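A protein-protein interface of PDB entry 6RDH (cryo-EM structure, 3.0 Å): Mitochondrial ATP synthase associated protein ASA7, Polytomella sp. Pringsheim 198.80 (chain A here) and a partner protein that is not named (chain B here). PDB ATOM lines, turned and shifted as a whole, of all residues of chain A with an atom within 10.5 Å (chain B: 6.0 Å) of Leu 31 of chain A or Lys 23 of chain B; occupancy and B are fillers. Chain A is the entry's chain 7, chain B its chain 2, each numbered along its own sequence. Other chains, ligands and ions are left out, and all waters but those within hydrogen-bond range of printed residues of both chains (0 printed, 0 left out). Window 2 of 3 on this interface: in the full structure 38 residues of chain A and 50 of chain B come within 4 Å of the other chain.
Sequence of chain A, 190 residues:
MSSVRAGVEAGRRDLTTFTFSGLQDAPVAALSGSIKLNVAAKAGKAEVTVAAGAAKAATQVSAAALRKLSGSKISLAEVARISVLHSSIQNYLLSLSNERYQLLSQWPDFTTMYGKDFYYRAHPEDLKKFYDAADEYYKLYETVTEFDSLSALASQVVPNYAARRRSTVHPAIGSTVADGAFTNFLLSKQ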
ATOM      1  N   ALA A  26     -24.278  -7.866  -6.280  1.00  0.00           N
ATOM      2  CA  ALA A  26     -25.182  -7.351  -5.286  1.00  0.00           C
ATOM      3  C   ALA A  26     -24.982  -8.114  -3.981  1.00  0.00           C
ATOM      4  O   ALA A  26     -24.342  -9.167  -3.965  1.00  0.00           O
ATOM      5  CB  ALA A  26     -26.619  -7.479  -5.783  1.00  0.00           C
ATOM      6  N   PRO A  27     -25.463  -7.573  -2.864  1.00  0.00           N
ATOM      7  CA  PRO A  27     -25.494  -8.355  -1.624  1.00  0.00           C
ATOM      8  C   PRO A  27     -26.359  -9.598  -1.754  1.00  0.00           C
ATOM      9  O   PRO A  27     -27.531  -9.528  -2.129  1.00  0.00           O
ATOM     10  CB  PRO A  27     -26.076  -7.374  -0.601  1.00  0.00           C
ATOM     11  CG  PRO A  27     -26.432  -6.148  -1.374  1.00  0.00           C
ATOM     12  CD  PRO A  27     -25.581  -6.140  -2.573  1.00  0.00           C
ATOM     13  N   VAL A  28     -25.757 -10.745  -1.438  1.00  0.00           N
ATOM     14  CA  VAL A  28     -26.465 -12.015  -1.492  1.00  0.00           C
ATOM     15  C   VAL A  28     -27.251 -12.303  -0.219  1.00  0.00           C
ATOM     16  O   VAL A  28     -28.157 -13.148  -0.242  1.00  0.00           O
ATOM     17  CB  VAL A  28     -25.485 -13.163  -1.775  1.00  0.00           C
ATOM     18  CG1 VAL A  28     -24.862 -12.988  -3.145  1.00  0.00           C
ATOM     19  CG2 VAL A  28     -24.404 -13.206  -0.714  1.00  0.00           C
ATOM     20  N   ALA A  29     -26.941 -11.621   0.883  1.00  0.00           N
ATOM     21  CA  ALA A  29     -27.633 -11.839   2.142  1.00  0.00           C
ATOM     22  C   ALA A  29     -27.572 -10.569   2.971  1.00  0.00           C
ATOM     23  O   ALA A  29     -26.731  -9.697   2.742  1.00  0.00           O
ATOM     24  CB  ALA A  29     -27.028 -13.010   2.922  1.00  0.00           C
ATOM     25  N   ALA A  30     -28.472 -10.477   3.945  1.00  0.00           N
ATOM     26  CA  ALA A  30     -28.433  -9.377   4.893  1.00  0.00           C
ATOM     27  C   ALA A  30     -27.268  -9.563   5.861  1.00  0.00           C
ATOM     28  O   ALA A  30     -26.681 -10.640   5.977  1.00  0.00           O
ATOM     29  CB  ALA A  30     -29.751  -9.274   5.655  1.00  0.00           C
ATOM     30  N   LEU A  31     -26.935  -8.489   6.571  1.00  0.00           N
ATOM     31  CA  LEU A  31     -25.778  -8.488   7.455  1.00  0.00           C
ATOM     32  C   LEU A  31     -26.124  -8.574   8.930  1.00  0.00           C
ATOM     33  O   LEU A  31     -25.315  -9.082   9.709  1.00  0.00           O
ATOM     34  CB  LEU A  31     -24.922  -7.239   7.213  1.00  0.00           C
ATOM     35  CG  LEU A  31     -23.720  -7.397   6.281  1.00  0.00           C
ATOM     36  CD1 LEU A  31     -22.689  -8.267   6.958  1.00  0.00           C
ATOM     37  CD2 LEU A  31     -24.090  -8.002   4.941  1.00  0.00           C
ATOM     38  N   SER A  32     -27.296  -8.106   9.334  1.00  0.00           N
ATOM     39  CA  SER A  32     -27.747  -8.238  10.705  1.00  0.00           C
ATOM     40  C   SER A  32     -29.022  -9.065  10.740  1.00  0.00           C
ATOM     41  O   SER A  32     -29.765  -9.143   9.758  1.00  0.00           O
ATOM     42  CB  SER A  32     -27.998  -6.872  11.347  1.00  0.00           C
ATOM     43  OG  SER A  32     -29.078  -6.214  10.714  1.00  0.00           O
ATOM     44  N   GLY A  33     -29.277  -9.670  11.894  1.00  0.00           N
ATOM     45  CA  GLY A  33     -30.462 -10.479  12.072  1.00  0.00           C
ATOM     46  C   GLY A  33     -31.748  -9.728  12.322  1.00  0.00           C
ATOM     47  O   GLY A  33     -32.768 -10.357  12.615  1.00  0.00           O
ATOM     48  N   SER A  34     -31.736  -8.400  12.225  1.00  0.00           N
ATOM     49  CA  SER A  34     -32.956  -7.633  12.436  1.00  0.00           C
ATOM     50  C   SER A  34     -33.898  -7.748  11.248  1.00  0.00           C
ATOM     51  O   SER A  34     -35.120  -7.676  11.413  1.00  0.00           O
ATOM     52  CB  SER A  34     -32.603  -6.176  12.698  1.00  0.00           C
ATOM     53  OG  SER A  34     -32.014  -5.612  11.545  1.00  0.00           O
ATOM     54  N   ILE A  35     -33.353  -7.918  10.052  1.00  0.00           N
ATOM     55  CA  ILE A  35     -34.155  -8.185   8.865  1.00  0.00           C
ATOM     56  C   ILE A  35     -33.431  -9.262   8.067  1.00  0.00           C
ATOM     57  O   ILE A  35     -32.197  -9.288   8.009  1.00  0.00           O
ATOM     58  CB  ILE A  35     -34.415  -6.893   8.053  1.00  0.00           C
ATOM     59  CG1 ILE A  35     -35.346  -7.127   6.876  1.00  0.00           C
ATOM     60  CG2 ILE A  35     -33.161  -6.278   7.537  1.00  0.00           C
ATOM     61  CD1 ILE A  35     -35.781  -5.836   6.234  1.00  0.00           C
ATOM     62  N   LYS A  36     -34.190 -10.211   7.538  1.00  0.00           N
ATOM     63  CA  LYS A  36     -33.612 -11.275   6.737  1.00  0.00           C
ATOM     64  C   LYS A  36     -33.905 -11.018   5.269  1.00  0.00           C
ATOM     65  O   LYS A  36     -35.025 -10.663   4.895  1.00  0.00           O
ATOM     66  CB  LYS A  36     -34.157 -12.637   7.162  1.00  0.00           C
ATOM     67  CG  LYS A  36     -33.665 -13.103   8.523  1.00  0.00           C
ATOM     68  CD  LYS A  36     -32.145 -13.092   8.589  1.00  0.00           C
ATOM     69  CE  LYS A  36     -31.648 -13.464   9.972  1.00  0.00           C
ATOM     70  NZ  LYS A  36     -30.183 -13.271  10.108  1.00  0.00           N
ATOM     71  N   LEU A  37     -32.886 -11.195   4.440  1.00  0.00           N
ATOM     72  CA  LEU A  37     -32.976 -10.879   3.024  1.00  0.00           C
ATOM     73  C   LEU A  37     -32.109 -11.867   2.268  1.00  0.00           C
ATOM     74  O   LEU A  37     -30.919 -12.000   2.565  1.00  0.00           O
ATOM     75  CB  LEU A  37     -32.529  -9.439   2.767  1.00  0.00           C
ATOM     76  CG  LEU A  37     -32.145  -8.932   1.381  1.00  0.00           C
ATOM     77  CD1 LEU A  37     -33.225  -9.159   0.346  1.00  0.00           C
ATOM     78  CD2 LEU A  37     -31.901  -7.475   1.535  1.00  0.00           C
ATOM     79  N   ASN A  38     -32.705 -12.576   1.320  1.00  0.00           N
ATOM     80  CA  ASN A  38     -31.964 -13.494   0.472  1.00  0.00           C
ATOM     81  C   ASN A  38     -32.349 -13.242  -0.975  1.00  0.00           C
ATOM     82  O   ASN A  38     -33.513 -12.962  -1.275  1.00  0.00           O
ATOM     83  CB  ASN A  38     -32.232 -14.952   0.851  1.00  0.00           C
ATOM     84  CG  ASN A  38     -33.681 -15.337   0.683  1.00  0.00           C
ATOM     85  OD1 ASN A  38     -34.575 -14.567   1.020  1.00  0.00           O
ATOM     86  ND2 ASN A  38     -33.922 -16.527   0.152  1.00  0.00           N
ATOM     87  N   ALA A  51     -37.566 -10.332   4.656  1.00  0.00           N
ATOM     88  CA  ALA A  51     -38.207 -10.873   5.851  1.00  0.00           C
ATOM     89  C   ALA A  51     -37.914  -9.971   7.039  1.00  0.00           C
ATOM     90  O   ALA A  51     -36.791  -9.965   7.548  1.00  0.00           O
ATOM     91  CB  ALA A  51     -37.727 -12.296   6.129  1.00  0.00           C
ATOM     92  N   SER B  21     -27.334   0.222  14.555  1.00  0.00           N
ATOM     93  CA  SER B  21     -25.966   0.101  14.089  1.00  0.00           C
ATOM     94  C   SER B  21     -25.955  -0.008  12.575  1.00  0.00           C
ATOM     95  O   SER B  21     -26.997  -0.055  11.927  1.00  0.00           O
ATOM     96  CB  SER B  21     -25.267  -1.104  14.705  1.00  0.00           C
ATOM     97  OG  SER B  21     -24.090  -1.408  13.971  1.00  0.00           O
ATOM     98  N   ALA B  22     -24.752  -0.099  12.010  1.00  0.00           N
ATOM     99  CA  ALA B  22     -24.587   0.104  10.578  1.00  0.00           C
ATOM    100  C   ALA B  22     -25.098  -1.059   9.751  1.00  0.00           C
ATOM    101  O   ALA B  22     -25.499  -0.856   8.602  1.00  0.00           O
ATOM    102  CB  ALA B  22     -23.132   0.324  10.255  1.00  0.00           C
ATOM    103  N   LYS B  23     -25.066  -2.275  10.295  1.00  0.00           N
ATOM    104  CA  LYS B  23     -25.530  -3.424   9.531  1.00  0.00           C
ATOM    105  C   LYS B  23     -27.028  -3.348   9.296  1.00  0.00           C
ATOM    106  O   LYS B  23     -27.499  -3.666   8.197  1.00  0.00           O
ATOM    107  CB  LYS B  23     -25.157  -4.717  10.242  1.00  0.00           C
ATOM    108  CG  LYS B  23     -23.670  -4.994  10.218  1.00  0.00           C
ATOM    109  CD  LYS B  23     -23.338  -6.336  10.823  1.00  0.00           C
ATOM    110  CE  LYS B  23     -21.899  -6.700  10.530  1.00  0.00           C
ATOM    111  NZ  LYS B  23     -20.973  -5.589  10.886  1.00  0.00           N
ATOM    112  N   GLU B  24     -27.780  -2.879  10.295  1.00  0.00           N
ATOM    113  CA  GLU B  24     -29.216  -2.695  10.125  1.00  0.00           C
ATOM    114  C   GLU B  24     -29.518  -1.601   9.113  1.00  0.00           C
ATOM    115  O   GLU B  24     -30.467  -1.722   8.334  1.00  0.00           O
ATOM    116  CB  GLU B  24     -29.871  -2.369  11.468  1.00  0.00           C
ATOM    117  CG  GLU B  24     -29.748  -3.440  12.545  1.00  0.00           C
ATOM    118  CD  GLU B  24     -28.553  -3.227  13.453  1.00  0.00           C
ATOM    119  OE1 GLU B  24     -27.515  -2.748  12.961  1.00  0.00           O
ATOM    120  OE2 GLU B  24     -28.650  -3.533  14.661  1.00  0.00           O
ATOM    121  N   VAL B  25     -28.698  -0.545   9.086  1.00  0.00           N
ATOM    122  CA  VAL B  25     -28.863   0.506   8.082  1.00  0.00           C
ATOM    123  C   VAL B  25     -28.611  -0.047   6.690  1.00  0.00           C
ATOM    124  O   VAL B  25     -29.369   0.224   5.752  1.00  0.00           O
ATOM    125  CB  VAL B  25     -27.925   1.689   8.364  1.00  0.00           C
ATOM    126  CG1 VAL B  25     -28.264   2.813   7.439  1.00  0.00           C
ATOM    127  CG2 VAL B  25     -28.046   2.148   9.780  1.00  0.00           C
ATOM    128  N   SER B  26     -27.550  -0.847   6.546  1.00  0.00           N
ATOM    129  CA  SER B  26     -27.161  -1.358   5.238  1.00  0.00           C
ATOM    130  C   SER B  26     -28.207  -2.308   4.685  1.00  0.00           C
ATOM    131  O   SER B  26     -28.634  -2.160   3.537  1.00  0.00           O
ATOM    132  CB  SER B  26     -25.813  -2.057   5.326  1.00  0.00           C
ATOM    133  OG  SER B  26     -25.923  -3.267   6.046  1.00  0.00           O
ATOM    134  N   ASP B  27     -28.663  -3.272   5.488  1.00  0.00           N
ATOM    135  CA  ASP B  27     -29.675  -4.164   4.942  1.00  0.00           C
ATOM    136  C   ASP B  27     -31.054  -3.521   4.867  1.00  0.00           C
ATOM    137  O   ASP B  27     -31.859  -3.959   4.046  1.00  0.00           O
ATOM    138  CB  ASP B  27     -29.748  -5.495   5.702  1.00  0.00           C
ATOM    139  CG  ASP B  27     -29.782  -5.335   7.201  1.00  0.00           C
ATOM    140  OD1 ASP B  27     -29.061  -6.082   7.893  1.00  0.00           O
ATOM    141  OD2 ASP B  27     -30.504  -4.464   7.708  1.00  0.00           O
ATOM    142  N   ALA B  28     -31.334  -2.466   5.642  1.00  0.00           N
ATOM    143  CA  ALA B  28     -32.570  -1.724   5.425  1.00  0.00           C
ATOM    144  C   ALA B  28     -32.524  -0.973   4.104  1.00  0.00           C
ATOM    145  O   ALA B  28     -33.527  -0.903   3.390  1.00  0.00           O
ATOM    146  CB  ALA B  28     -32.820  -0.760   6.579  1.00  0.00           C
ATOM    147  N   ASP B  56     -19.675   2.380  13.725  1.00  0.00           N
ATOM    148  CA  ASP B  56     -19.088   1.115  13.317  1.00  0.00           C
ATOM    149  C   ASP B  56     -19.309   0.950  11.827  1.00  0.00           C
ATOM    150  O   ASP B  56     -20.326   1.382  11.294  1.00  0.00           O
ATOM    151  CB  ASP B  56     -19.699  -0.053  14.089  1.00  0.00           C
ATOM    152  CG  ASP B  56     -21.198  -0.135  13.919  1.00  0.00           C
ATOM    153  OD1 ASP B  56     -21.841   0.919  13.759  1.00  0.00           O
ATOM    154  OD2 ASP B  56     -21.750  -1.253  13.975  1.00  0.00           O
ATOM    155  N   ASP B  58     -17.739  -1.966   8.702  1.00  0.00           N
ATOM    156  CA  ASP B  58     -16.861  -2.958   8.120  1.00  0.00           C
ATOM    157  C   ASP B  58     -16.946  -2.855   6.603  1.00  0.00           C
ATOM    158  O   ASP B  58     -17.497  -1.896   6.061  1.00  0.00           O
ATOM    159  CB  ASP B  58     -17.207  -4.352   8.648  1.00  0.00           C
ATOM    160  CG  ASP B  58     -18.680  -4.671   8.554  1.00  0.00           C
ATOM    161  OD1 ASP B  58     -19.454  -3.826   8.058  1.00  0.00           O
ATOM    162  OD2 ASP B  58     -19.065  -5.779   8.976  1.00  0.00           O
ATOM    163  N   ALA B  60     -18.450  -5.116   4.468  1.00  0.00           N
ATOM    164  CA  ALA B  60     -19.665  -5.642   3.860  1.00  0.00           C
ATOM    165  C   ALA B  60     -20.828  -4.674   3.988  1.00  0.00           C
ATOM    166  O   ALA B  60     -21.548  -4.443   3.013  1.00  0.00           O
ATOM    167  CB  ALA B  60     -20.020  -6.984   4.490  1.00  0.00           C
ATOM    168  N   SER B  61     -21.016  -4.079   5.169  1.00  0.00           N
ATOM    169  CA  SER B  61     -22.149  -3.181   5.373  1.00  0.00           C
ATOM    170  C   SER B  61     -21.965  -1.875   4.617  1.00  0.00           C
ATOM    171  O   SER B  61     -22.921  -1.360   4.028  1.00  0.00           O
ATOM    172  CB  SER B  61     -22.347  -2.917   6.857  1.00  0.00           C
ATOM    173  OG  SER B  61     -21.184  -2.338   7.413  1.00  0.00           O
ATOM    174  N   ASN B  64     -22.603  -2.771   0.848  1.00  0.00           N
ATOM    175  CA  ASN B  64     -24.009  -2.949   0.493  1.00  0.00           C
ATOM    176  C   ASN B  64     -24.799  -1.664   0.656  1.00  0.00           C
ATOM    177  O   ASN B  64     -25.752  -1.435  -0.097  1.00  0.00           O
ATOM    178  CB  ASN B  64     -24.661  -4.051   1.320  1.00  0.00           C
ATOM    179  CG  ASN B  64     -23.892  -5.343   1.281  1.00  0.00           C
ATOM    180  OD1 ASN B  64     -23.814  -6.051   2.278  1.00  0.00           O
ATOM    181  ND2 ASN B  64     -23.296  -5.648   0.137  1.00  0.00           N
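The backbone NH (N) of Leu 31 of chain A is in hydrogen-bond range of the side-chain carboxylate (OD1) of Asp 27 of chain B, 3.5 Å away.
OD1 of Asp 27 of chain B is in hydrogen-bond range of OG of Ser 32 of chain A (2.8 Å).
N of Ser 21 of chain B sits close to OE1 of Glu 24 of chain B (3.4 Å).
O of Lys 23 of chain B is in hydrogen-bond range of OG of Ser 26 of chain B.
OD2 of Asp 58 of chain B is in salt-bridge range of NZ of Lys 23 of chain B (2.7 Å).
The side-chain hydroxyl (OG) of Ser 34 of chain A lies within hydrogen-bond range of the side-chain hydroxyl (OG) of Ser 32 of chain A, at 3.1 Å.
OD1 of Asn 64 of chain B sits close to O of Ala 60 of chain B, at 2.9 Å.
The backbone NH (N) of Ala 30 of chain A lies within hydrogen-bond range of the backbone carbonyl oxygen (O) of Leu 37 of chain A (3.2 Å).
Among the printed residues, pairs that only touch across the chains: Ile 35 of chain A with Asp 27 of chain B (3.2 Å), Ser 34 of chain A with Glu 24 of chain B (3.3 Å), Leu 31 of chain A with Asn 64 of chain B (3.3 Å), Pro 27 of chain A with Asn 64 of chain B (3.4 Å), Ser 32 of chain A with Glu 24 of chain B (3.4 Å), Leu 31 of chain A with Lys 23 of chain B (3.6 Å), Ser 32 of chain A with Lys 23 of chain B (3.7 Å), Ala 30 of chain A with Asp 27 of chain B (3.8 Å) and Leu 31 of chain A with Ala 60 of chain B (3.9 Å).
Of the printed residues of chain B, Ala 30 of chain A touches Asp 27.
Of the printed residues of chain B, Ser 32 of chain A touches Lys 23, Glu 24 and Asp 27.
Of the printed residues of chain B, Ser 34 of chain A touches Glu 24 (3.3 Å).
Of the printed residues of chain B, Ile 35 of chain A touches Asp 27 (3.2 Å).
No residue of chain A comes within 4 Å of Ser 21 of chain B.
No residue of chain A comes within 4 Å of Ala 22 of chain B.
Of chain A, only Leu 31 and Ser 32 come within 4 Å of Lys 23 of chain B.
Glu 24 of chain B touches just these residues of chain A: Ser 32 (3.4 Å) and Ser 34 (3.3 Å).
No residue of chain A comes within 4 Å of Ser 26 of chain B.
Of the printed residues of chain A, Asp 27 of chain B touches Ala 30, Leu 31, Ser 32 and Ile 35.
Of the printed residues of chain A, Asn 64 of chain B touches Pro 27 (3.4 Å) and Leu 31 (3.3 Å).
The nearest residue of chain B that does not touch Leu 31 of chain A is Ser 26 of chain B (4.3 Å).
Of the 14 printed residues of chain A, 6 touch a printed residue of chain B.
Hydrophobic or aromatic side chains of chain A that line the printed part of chain B: Pro 27, Ala 30, Leu 31 and Ile 35.
Printed residues of chain B that touch a printed residue of chain A: Lys 23, Glu 24, Asp 27, Ala 60 and Asn 64.
Among the printed residues, no Asp or Glu carboxylate lies within 4 Å of a Lys or Arg side-chain nitrogen of the other chain.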
